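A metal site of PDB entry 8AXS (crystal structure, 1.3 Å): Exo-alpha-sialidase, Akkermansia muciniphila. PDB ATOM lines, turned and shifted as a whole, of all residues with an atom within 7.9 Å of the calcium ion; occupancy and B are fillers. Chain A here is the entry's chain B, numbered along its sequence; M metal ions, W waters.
The calcium ion is bound by the side-chain carboxylate (OD1) of Asp 279 (2.3 Å), water W3 (2.4 Å), the side-chain carboxylate (OE2) of Glu 278 (2.4 Å), water W1 (2.4 Å), the side-chain carboxylate (OE1) of Glu 268 (2.4 Å), water W2 (2.5 Å) and the side-chain carboxylate (OE2) of Glu 268 (2.5 Å).
The calcium ion has seven donor atoms within binding distance.
The backbone NH of Val 280 lies close to the side-chain carboxylate of Glu 278 (3.3 Å).
The backbone NH (N) of Glu 268 sits at hydrogen-bond distance from a ring nitrogen (ND1) of His 186 (3.0 Å).
Water W2 bridges the side-chain carboxylate (OE1) of Glu 278 (2.7 Å) and the backbone NH (N) of Trp 191 (3.0 Å).
Water W1 lies within hydrogen-bond range of the backbone carbonyl oxygen of Val 189 (2.8 Å), the backbone carbonyl oxygen of Ala 272 (3.2 Å) and the backbone NH of Trp 191 (3.4 Å).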
ATOM      1  N   HIS A 180       4.934  28.388  -3.774  1.00  0.00           N
ATOM      2  CA  HIS A 180       6.302  28.274  -3.327  1.00  0.00           C
ATOM      3  C   HIS A 180       6.866  26.963  -3.861  1.00  0.00           C
ATOM      4  O   HIS A 180       6.169  25.948  -3.918  1.00  0.00           O
ATOM      5  CB  HIS A 180       6.352  28.289  -1.805  1.00  0.00           C
ATOM      6  CG  HIS A 180       7.717  28.012  -1.235  1.00  0.00           C
ATOM      7  ND1 HIS A 180       8.011  26.870  -0.532  1.00  0.00           N
ATOM      8  CD2 HIS A 180       8.858  28.750  -1.257  1.00  0.00           C
ATOM      9  CE1 HIS A 180       9.271  26.901  -0.159  1.00  0.00           C
ATOM     10  NE2 HIS A 180       9.810  28.019  -0.584  1.00  0.00           N
ATOM     11  N   HIS A 186      14.919  24.900   2.043  1.00  0.00           N
ATOM     12  CA  HIS A 186      13.650  24.271   2.401  1.00  0.00           C
ATOM     13  C   HIS A 186      13.696  22.770   2.172  1.00  0.00           C
ATOM     14  O   HIS A 186      14.314  22.269   1.209  1.00  0.00           O
ATOM     15  CB  HIS A 186      12.546  24.861   1.538  1.00  0.00           C
ATOM     16  CG  HIS A 186      12.360  26.326   1.718  1.00  0.00           C
ATOM     17  ND1 HIS A 186      11.766  26.852   2.846  1.00  0.00           N
ATOM     18  CD2 HIS A 186      12.665  27.364   0.928  1.00  0.00           C
ATOM     19  CE1 HIS A 186      11.725  28.157   2.725  1.00  0.00           C
ATOM     20  NE2 HIS A 186      12.276  28.500   1.579  1.00  0.00           N
ATOM     21  N   GLY A 188      10.544  21.281   2.199  1.00  0.00           N
ATOM     22  CA  GLY A 188       9.123  21.137   1.943  1.00  0.00           C
ATOM     23  C   GLY A 188       8.599  22.458   1.449  1.00  0.00           C
ATOM     24  O   GLY A 188       9.343  23.420   1.276  1.00  0.00           O
ATOM     25  N   VAL A 189       7.279  22.491   1.186  1.00  0.00           N
ATOM     26  CA  VAL A 189       6.623  23.637   0.588  1.00  0.00           C
ATOM     27  C   VAL A 189       5.886  24.476   1.633  1.00  0.00           C
ATOM     28  O   VAL A 189       5.164  23.947   2.486  1.00  0.00           O
ATOM     29  CB  VAL A 189       5.674  23.284  -0.572  1.00  0.00           C
ATOM     30  CG1 VAL A 189       6.423  22.616  -1.705  1.00  0.00           C
ATOM     31  CG2 VAL A 189       4.505  22.460  -0.102  1.00  0.00           C
ATOM     32  N   ARG A 190       5.958  25.780   1.438  1.00  0.00           N
ATOM     33  CA  ARG A 190       5.198  26.713   2.254  1.00  0.00           C
ATOM     34  C   ARG A 190       3.703  26.579   1.938  1.00  0.00           C
ATOM     35  O   ARG A 190       3.299  26.195   0.824  1.00  0.00           O
ATOM     36  CB  ARG A 190       5.620  28.138   1.929  1.00  0.00           C
ATOM     37  CG  ARG A 190       7.000  28.549   2.435  1.00  0.00           C
ATOM     38  CD  ARG A 190       7.237  30.028   2.187  1.00  0.00           C
ATOM     39  NE  ARG A 190       8.535  30.475   2.688  1.00  0.00           N
ATOM     40  CZ  ARG A 190       9.296  31.397   2.133  1.00  0.00           C
ATOM     41  NH1 ARG A 190       8.915  32.041   1.025  1.00  0.00           N
ATOM     42  NH2 ARG A 190      10.464  31.705   2.692  1.00  0.00           N
ATOM     43  N   TRP A 191       2.890  26.893   2.949  1.00  0.00           N
ATOM     44  CA  TRP A 191       1.454  27.071   2.766  1.00  0.00           C
ATOM     45  C   TRP A 191       1.217  27.976   1.563  1.00  0.00           C
ATOM     46  O   TRP A 191       1.780  29.084   1.479  1.00  0.00           O
ATOM     47  CB  TRP A 191       0.909  27.750   4.036  1.00  0.00           C
ATOM     48  CG  TRP A 191      -0.571  27.977   4.074  1.00  0.00           C
ATOM     49  CD1 TRP A 191      -1.540  27.311   3.403  1.00  0.00           C
ATOM     50  CD2 TRP A 191      -1.242  28.930   4.916  1.00  0.00           C
ATOM     51  NE1 TRP A 191      -2.777  27.808   3.744  1.00  0.00           N
ATOM     52  CE2 TRP A 191      -2.625  28.789   4.698  1.00  0.00           C
ATOM     53  CE3 TRP A 191      -0.805  29.879   5.846  1.00  0.00           C
ATOM     54  CZ2 TRP A 191      -3.569  29.576   5.350  1.00  0.00           C
ATOM     55  CZ3 TRP A 191      -1.764  30.683   6.495  1.00  0.00           C
ATOM     56  CH2 TRP A 191      -3.121  30.509   6.233  1.00  0.00           C
ATOM     57  N   PHE A 192       0.365  27.533   0.637  1.00  0.00           N
ATOM     58  CA  PHE A 192       0.029  28.324  -0.545  1.00  0.00           C
ATOM     59  C   PHE A 192      -1.095  29.312  -0.244  1.00  0.00           C
ATOM     60  O   PHE A 192      -2.204  28.931   0.129  1.00  0.00           O
ATOM     61  CB  PHE A 192      -0.386  27.431  -1.701  1.00  0.00           C
ATOM     62  CG  PHE A 192      -0.740  28.177  -2.951  1.00  0.00           C
ATOM     63  CD1 PHE A 192       0.060  29.212  -3.418  1.00  0.00           C
ATOM     64  CD2 PHE A 192      -1.899  27.882  -3.646  1.00  0.00           C
ATOM     65  CE1 PHE A 192      -0.272  29.920  -4.589  1.00  0.00           C
ATOM     66  CE2 PHE A 192      -2.237  28.582  -4.803  1.00  0.00           C
ATOM     67  CZ  PHE A 192      -1.436  29.600  -5.273  1.00  0.00           C
ATOM     68  N   LEU A 243       3.104  35.273   4.043  1.00  0.00           N
ATOM     69  CA  LEU A 243       1.942  34.736   4.721  1.00  0.00           C
ATOM     70  C   LEU A 243       1.575  35.605   5.925  1.00  0.00           C
ATOM     71  O   LEU A 243       1.123  35.119   6.959  1.00  0.00           O
ATOM     72  CB  LEU A 243       2.156  33.249   5.095  1.00  0.00           C
ATOM     73  CG  LEU A 243       2.350  32.367   3.829  1.00  0.00           C
ATOM     74  CD1 LEU A 243       2.982  31.020   4.225  1.00  0.00           C
ATOM     75  CD2 LEU A 243       1.007  32.137   3.096  1.00  0.00           C
ATOM     76  N   ALA A 265      10.534  33.782   7.475  1.00  0.00           N
ATOM     77  CA  ALA A 265      10.242  32.550   8.195  1.00  0.00           C
ATOM     78  C   ALA A 265      11.439  31.612   8.150  1.00  0.00           C
ATOM     79  O   ALA A 265      12.299  31.720   7.280  1.00  0.00           O
ATOM     80  CB  ALA A 265       9.044  31.864   7.562  1.00  0.00           C
ATOM     81  N   LEU A 266      11.490  30.700   9.112  1.00  0.00           N
ATOM     82  CA  LEU A 266      12.501  29.656   9.037  1.00  0.00           C
ATOM     83  C   LEU A 266      12.231  28.803   7.785  1.00  0.00           C
ATOM     84  O   LEU A 266      11.074  28.631   7.386  1.00  0.00           O
ATOM     85  CB  LEU A 266      12.466  28.737  10.271  1.00  0.00           C
ATOM     86  CG  LEU A 266      13.158  29.249  11.518  1.00  0.00           C
ATOM     87  CD1 LEU A 266      12.798  28.391  12.707  1.00  0.00           C
ATOM     88  CD2 LEU A 266      14.665  29.363  11.390  1.00  0.00           C
ATOM     89  N   PRO A 267      13.272  28.171   7.233  1.00  0.00           N
ATOM     90  CA  PRO A 267      13.068  27.230   6.140  1.00  0.00           C
ATOM     91  C   PRO A 267      12.083  26.131   6.518  1.00  0.00           C
ATOM     92  O   PRO A 267      12.044  25.652   7.644  1.00  0.00           O
ATOM     93  CB  PRO A 267      14.482  26.663   5.873  1.00  0.00           C
ATOM     94  CG  PRO A 267      15.434  27.719   6.374  1.00  0.00           C
ATOM     95  CD  PRO A 267      14.700  28.357   7.566  1.00  0.00           C
ATOM     96  N   GLU A 268      11.346  25.653   5.513  1.00  0.00           N
ATOM     97  CA  GLU A 268      10.412  24.563   5.726  1.00  0.00           C
ATOM     98  C   GLU A 268      11.133  23.281   6.110  1.00  0.00           C
ATOM     99  O   GLU A 268      12.238  22.983   5.621  1.00  0.00           O
ATOM    100  CB  GLU A 268       9.614  24.320   4.436  1.00  0.00           C
ATOM    101  CG  GLU A 268       8.705  25.469   4.048  1.00  0.00           C
ATOM    102  CD  GLU A 268       7.620  25.723   5.113  1.00  0.00           C
ATOM    103  OE1 GLU A 268       7.153  24.782   5.809  1.00  0.00           O
ATOM    104  OE2 GLU A 268       7.239  26.906   5.307  1.00  0.00           O
ATOM    105  N   ASN A 269      10.508  22.509   6.989  1.00  0.00           N
ATOM    106  CA  ASN A 269      11.082  21.268   7.472  1.00  0.00           C
ATOM    107  C   ASN A 269      10.563  20.095   6.655  1.00  0.00           C
ATOM    108  O   ASN A 269       9.873  20.237   5.658  1.00  0.00           O
ATOM    109  CB  ASN A 269      10.842  21.149   8.998  1.00  0.00           C
ATOM    110  CG  ASN A 269       9.426  20.935   9.337  1.00  0.00           C
ATOM    111  OD1 ASN A 269       8.667  20.293   8.617  1.00  0.00           O
ATOM    112  ND2 ASN A 269       9.014  21.478  10.506  1.00  0.00           N
ATOM    113  N   THR A 271       8.499  17.757   7.377  1.00  0.00           N
ATOM    114  CA  THR A 271       7.109  17.381   7.634  1.00  0.00           C
ATOM    115  C   THR A 271       6.181  18.577   7.407  1.00  0.00           C
ATOM    116  O   THR A 271       5.202  18.764   8.116  1.00  0.00           O
ATOM    117  CB  THR A 271       6.935  16.829   9.059  1.00  0.00           C
ATOM    118  OG1 THR A 271       7.320  17.797  10.042  1.00  0.00           O
ATOM    119  CG2 THR A 271       7.735  15.554   9.302  1.00  0.00           C
ATOM    120  N   ALA A 272       6.506  19.392   6.419  1.00  0.00           N
ATOM    121  CA  ALA A 272       5.772  20.654   6.222  1.00  0.00           C
ATOM    122  C   ALA A 272       4.363  20.481   5.673  1.00  0.00           C
ATOM    123  O   ALA A 272       3.572  21.430   5.731  1.00  0.00           O
ATOM    124  CB  ALA A 272       6.577  21.585   5.366  1.00  0.00           C
ATOM    125  N   GLY A 273       4.050  19.321   5.101  1.00  0.00           N
ATOM    126  CA  GLY A 273       2.753  19.133   4.460  1.00  0.00           C
ATOM    127  C   GLY A 273       2.762  19.505   2.994  1.00  0.00           C
ATOM    128  O   GLY A 273       3.783  19.841   2.404  1.00  0.00           O
ATOM    129  N   GLY A 275       1.146  21.962   1.488  1.00  0.00           N
ATOM    130  CA  GLY A 275       0.939  23.347   1.136  1.00  0.00           C
ATOM    131  C   GLY A 275      -0.498  23.803   1.140  1.00  0.00           C
ATOM    132  O   GLY A 275      -0.747  24.994   0.948  1.00  0.00           O
ATOM    133  N   TRP A 277      -2.512  23.803   3.814  1.00  0.00           N
ATOM    134  CA  TRP A 277      -2.578  24.575   5.048  1.00  0.00           C
ATOM    135  C   TRP A 277      -1.174  24.708   5.629  1.00  0.00           C
ATOM    136  O   TRP A 277      -0.193  24.152   5.132  1.00  0.00           O
ATOM    137  CB  TRP A 277      -3.532  23.928   6.063  1.00  0.00           C
ATOM    138  CG  TRP A 277      -5.011  23.860   5.609  1.00  0.00           C
ATOM    139  CD1 TRP A 277      -5.676  22.743   5.210  1.00  0.00           C
ATOM    140  CD2 TRP A 277      -5.954  24.941   5.535  1.00  0.00           C
ATOM    141  NE1 TRP A 277      -6.971  23.057   4.901  1.00  0.00           N
ATOM    142  CE2 TRP A 277      -7.170  24.396   5.096  1.00  0.00           C
ATOM    143  CE3 TRP A 277      -5.894  26.314   5.804  1.00  0.00           C
ATOM    144  CZ2 TRP A 277      -8.321  25.172   4.897  1.00  0.00           C
ATOM    145  CZ3 TRP A 277      -7.030  27.088   5.625  1.00  0.00           C
ATOM    146  CH2 TRP A 277      -8.232  26.511   5.173  1.00  0.00           C
ATOM    147  N   GLU A 278      -1.081  25.529   6.658  1.00  0.00           N
ATOM    148  CA  GLU A 278       0.189  25.767   7.345  1.00  0.00           C
ATOM    149  C   GLU A 278       0.541  24.596   8.244  1.00  0.00           C
ATOM    150  O   GLU A 278      -0.343  23.901   8.746  1.00  0.00           O
ATOM    151  CB  GLU A 278       0.032  27.039   8.173  1.00  0.00           C
ATOM    152  CG  GLU A 278       1.287  27.591   8.780  1.00  0.00           C
ATOM    153  CD  GLU A 278       2.418  27.709   7.786  1.00  0.00           C
ATOM    154  OE1 GLU A 278       2.566  28.741   7.141  1.00  0.00           O
ATOM    155  OE2 GLU A 278       3.188  26.735   7.648  1.00  0.00           O
ATOM    156  N   ASP A 279       1.849  24.388   8.464  1.00  0.00           N
ATOM    157  CA  ASP A 279       2.321  23.488   9.518  1.00  0.00           C
ATOM    158  C   ASP A 279       2.674  24.257  10.790  1.00  0.00           C
ATOM    159  O   ASP A 279       2.234  23.886  11.888  1.00  0.00           O
ATOM    160  CB  ASP A 279       3.465  22.577   9.051  1.00  0.00           C
ATOM    161  CG  ASP A 279       4.762  23.285   8.757  1.00  0.00           C
ATOM    162  OD1 ASP A 279       4.737  24.387   8.125  1.00  0.00           O
ATOM    163  OD2 ASP A 279       5.817  22.698   9.117  1.00  0.00           O
ATOM    164  N   VAL A 280       3.428  25.350  10.683  1.00  0.00           N
ATOM    165  CA  VAL A 280       3.871  26.084  11.865  1.00  0.00           C
ATOM    166  C   VAL A 280       4.244  27.515  11.433  1.00  0.00           C
ATOM    167  O   VAL A 280       4.830  27.725  10.372  1.00  0.00           O
ATOM    168  CB  VAL A 280       5.043  25.355  12.578  1.00  0.00           C
ATOM    169  CG1 VAL A 280       6.281  25.368  11.756  1.00  0.00           C
ATOM    170  CG2 VAL A 280       5.288  26.024  13.933  1.00  0.00           C
ATOM    171  N   PHE A 281       3.928  28.479  12.303  1.00  0.00           N
ATOM    172  CA  PHE A 281       4.256  29.896  12.077  1.00  0.00           C
ATOM    173  C   PHE A 281       5.552  30.247  12.811  1.00  0.00           C
ATOM    174  O   PHE A 281       5.657  30.085  14.028  1.00  0.00           O
ATOM    175  CB  PHE A 281       3.143  30.817  12.576  1.00  0.00           C
ATOM    176  CG  PHE A 281       1.895  30.721  11.797  1.00  0.00           C
ATOM    177  CD1 PHE A 281       1.886  31.090  10.470  1.00  0.00           C
ATOM    178  CD2 PHE A 281       0.726  30.281  12.359  1.00  0.00           C
ATOM    179  CE1 PHE A 281       0.736  31.018   9.729  1.00  0.00           C
ATOM    180  CE2 PHE A 281      -0.455  30.212  11.580  1.00  0.00           C
ATOM    181  CZ  PHE A 281      -0.416  30.588  10.268  1.00  0.00           C
ATOM    182  N   THR A 282       6.566  30.708  12.065  1.00  0.00           N
ATOM    183  CA  THR A 282       7.856  31.106  12.626  1.00  0.00           C
ATOM    184  C   THR A 282       8.215  32.540  12.246  1.00  0.00           C
ATOM    185  O   THR A 282       9.401  32.895  12.268  1.00  0.00           O
ATOM    186  CB  THR A 282       8.981  30.143  12.227  1.00  0.00           C
ATOM    187  OG1 THR A 282       9.187  30.167  10.788  1.00  0.00           O
ATOM    188  CG2 THR A 282       8.688  28.742  12.688  1.00  0.00           C
HETATM  189 CA    CA M   1       5.241  26.060   6.588  1.00  0.00          CA
HETATM  190  O   HOH W   1       4.165  24.533   5.036  1.00  0.00           O
HETATM  191  O   HOH W   2       4.443  28.036   5.289  1.00  0.00           O
HETATM  192  O   HOH W   3       6.336  27.348   8.264  1.00  0.00           O
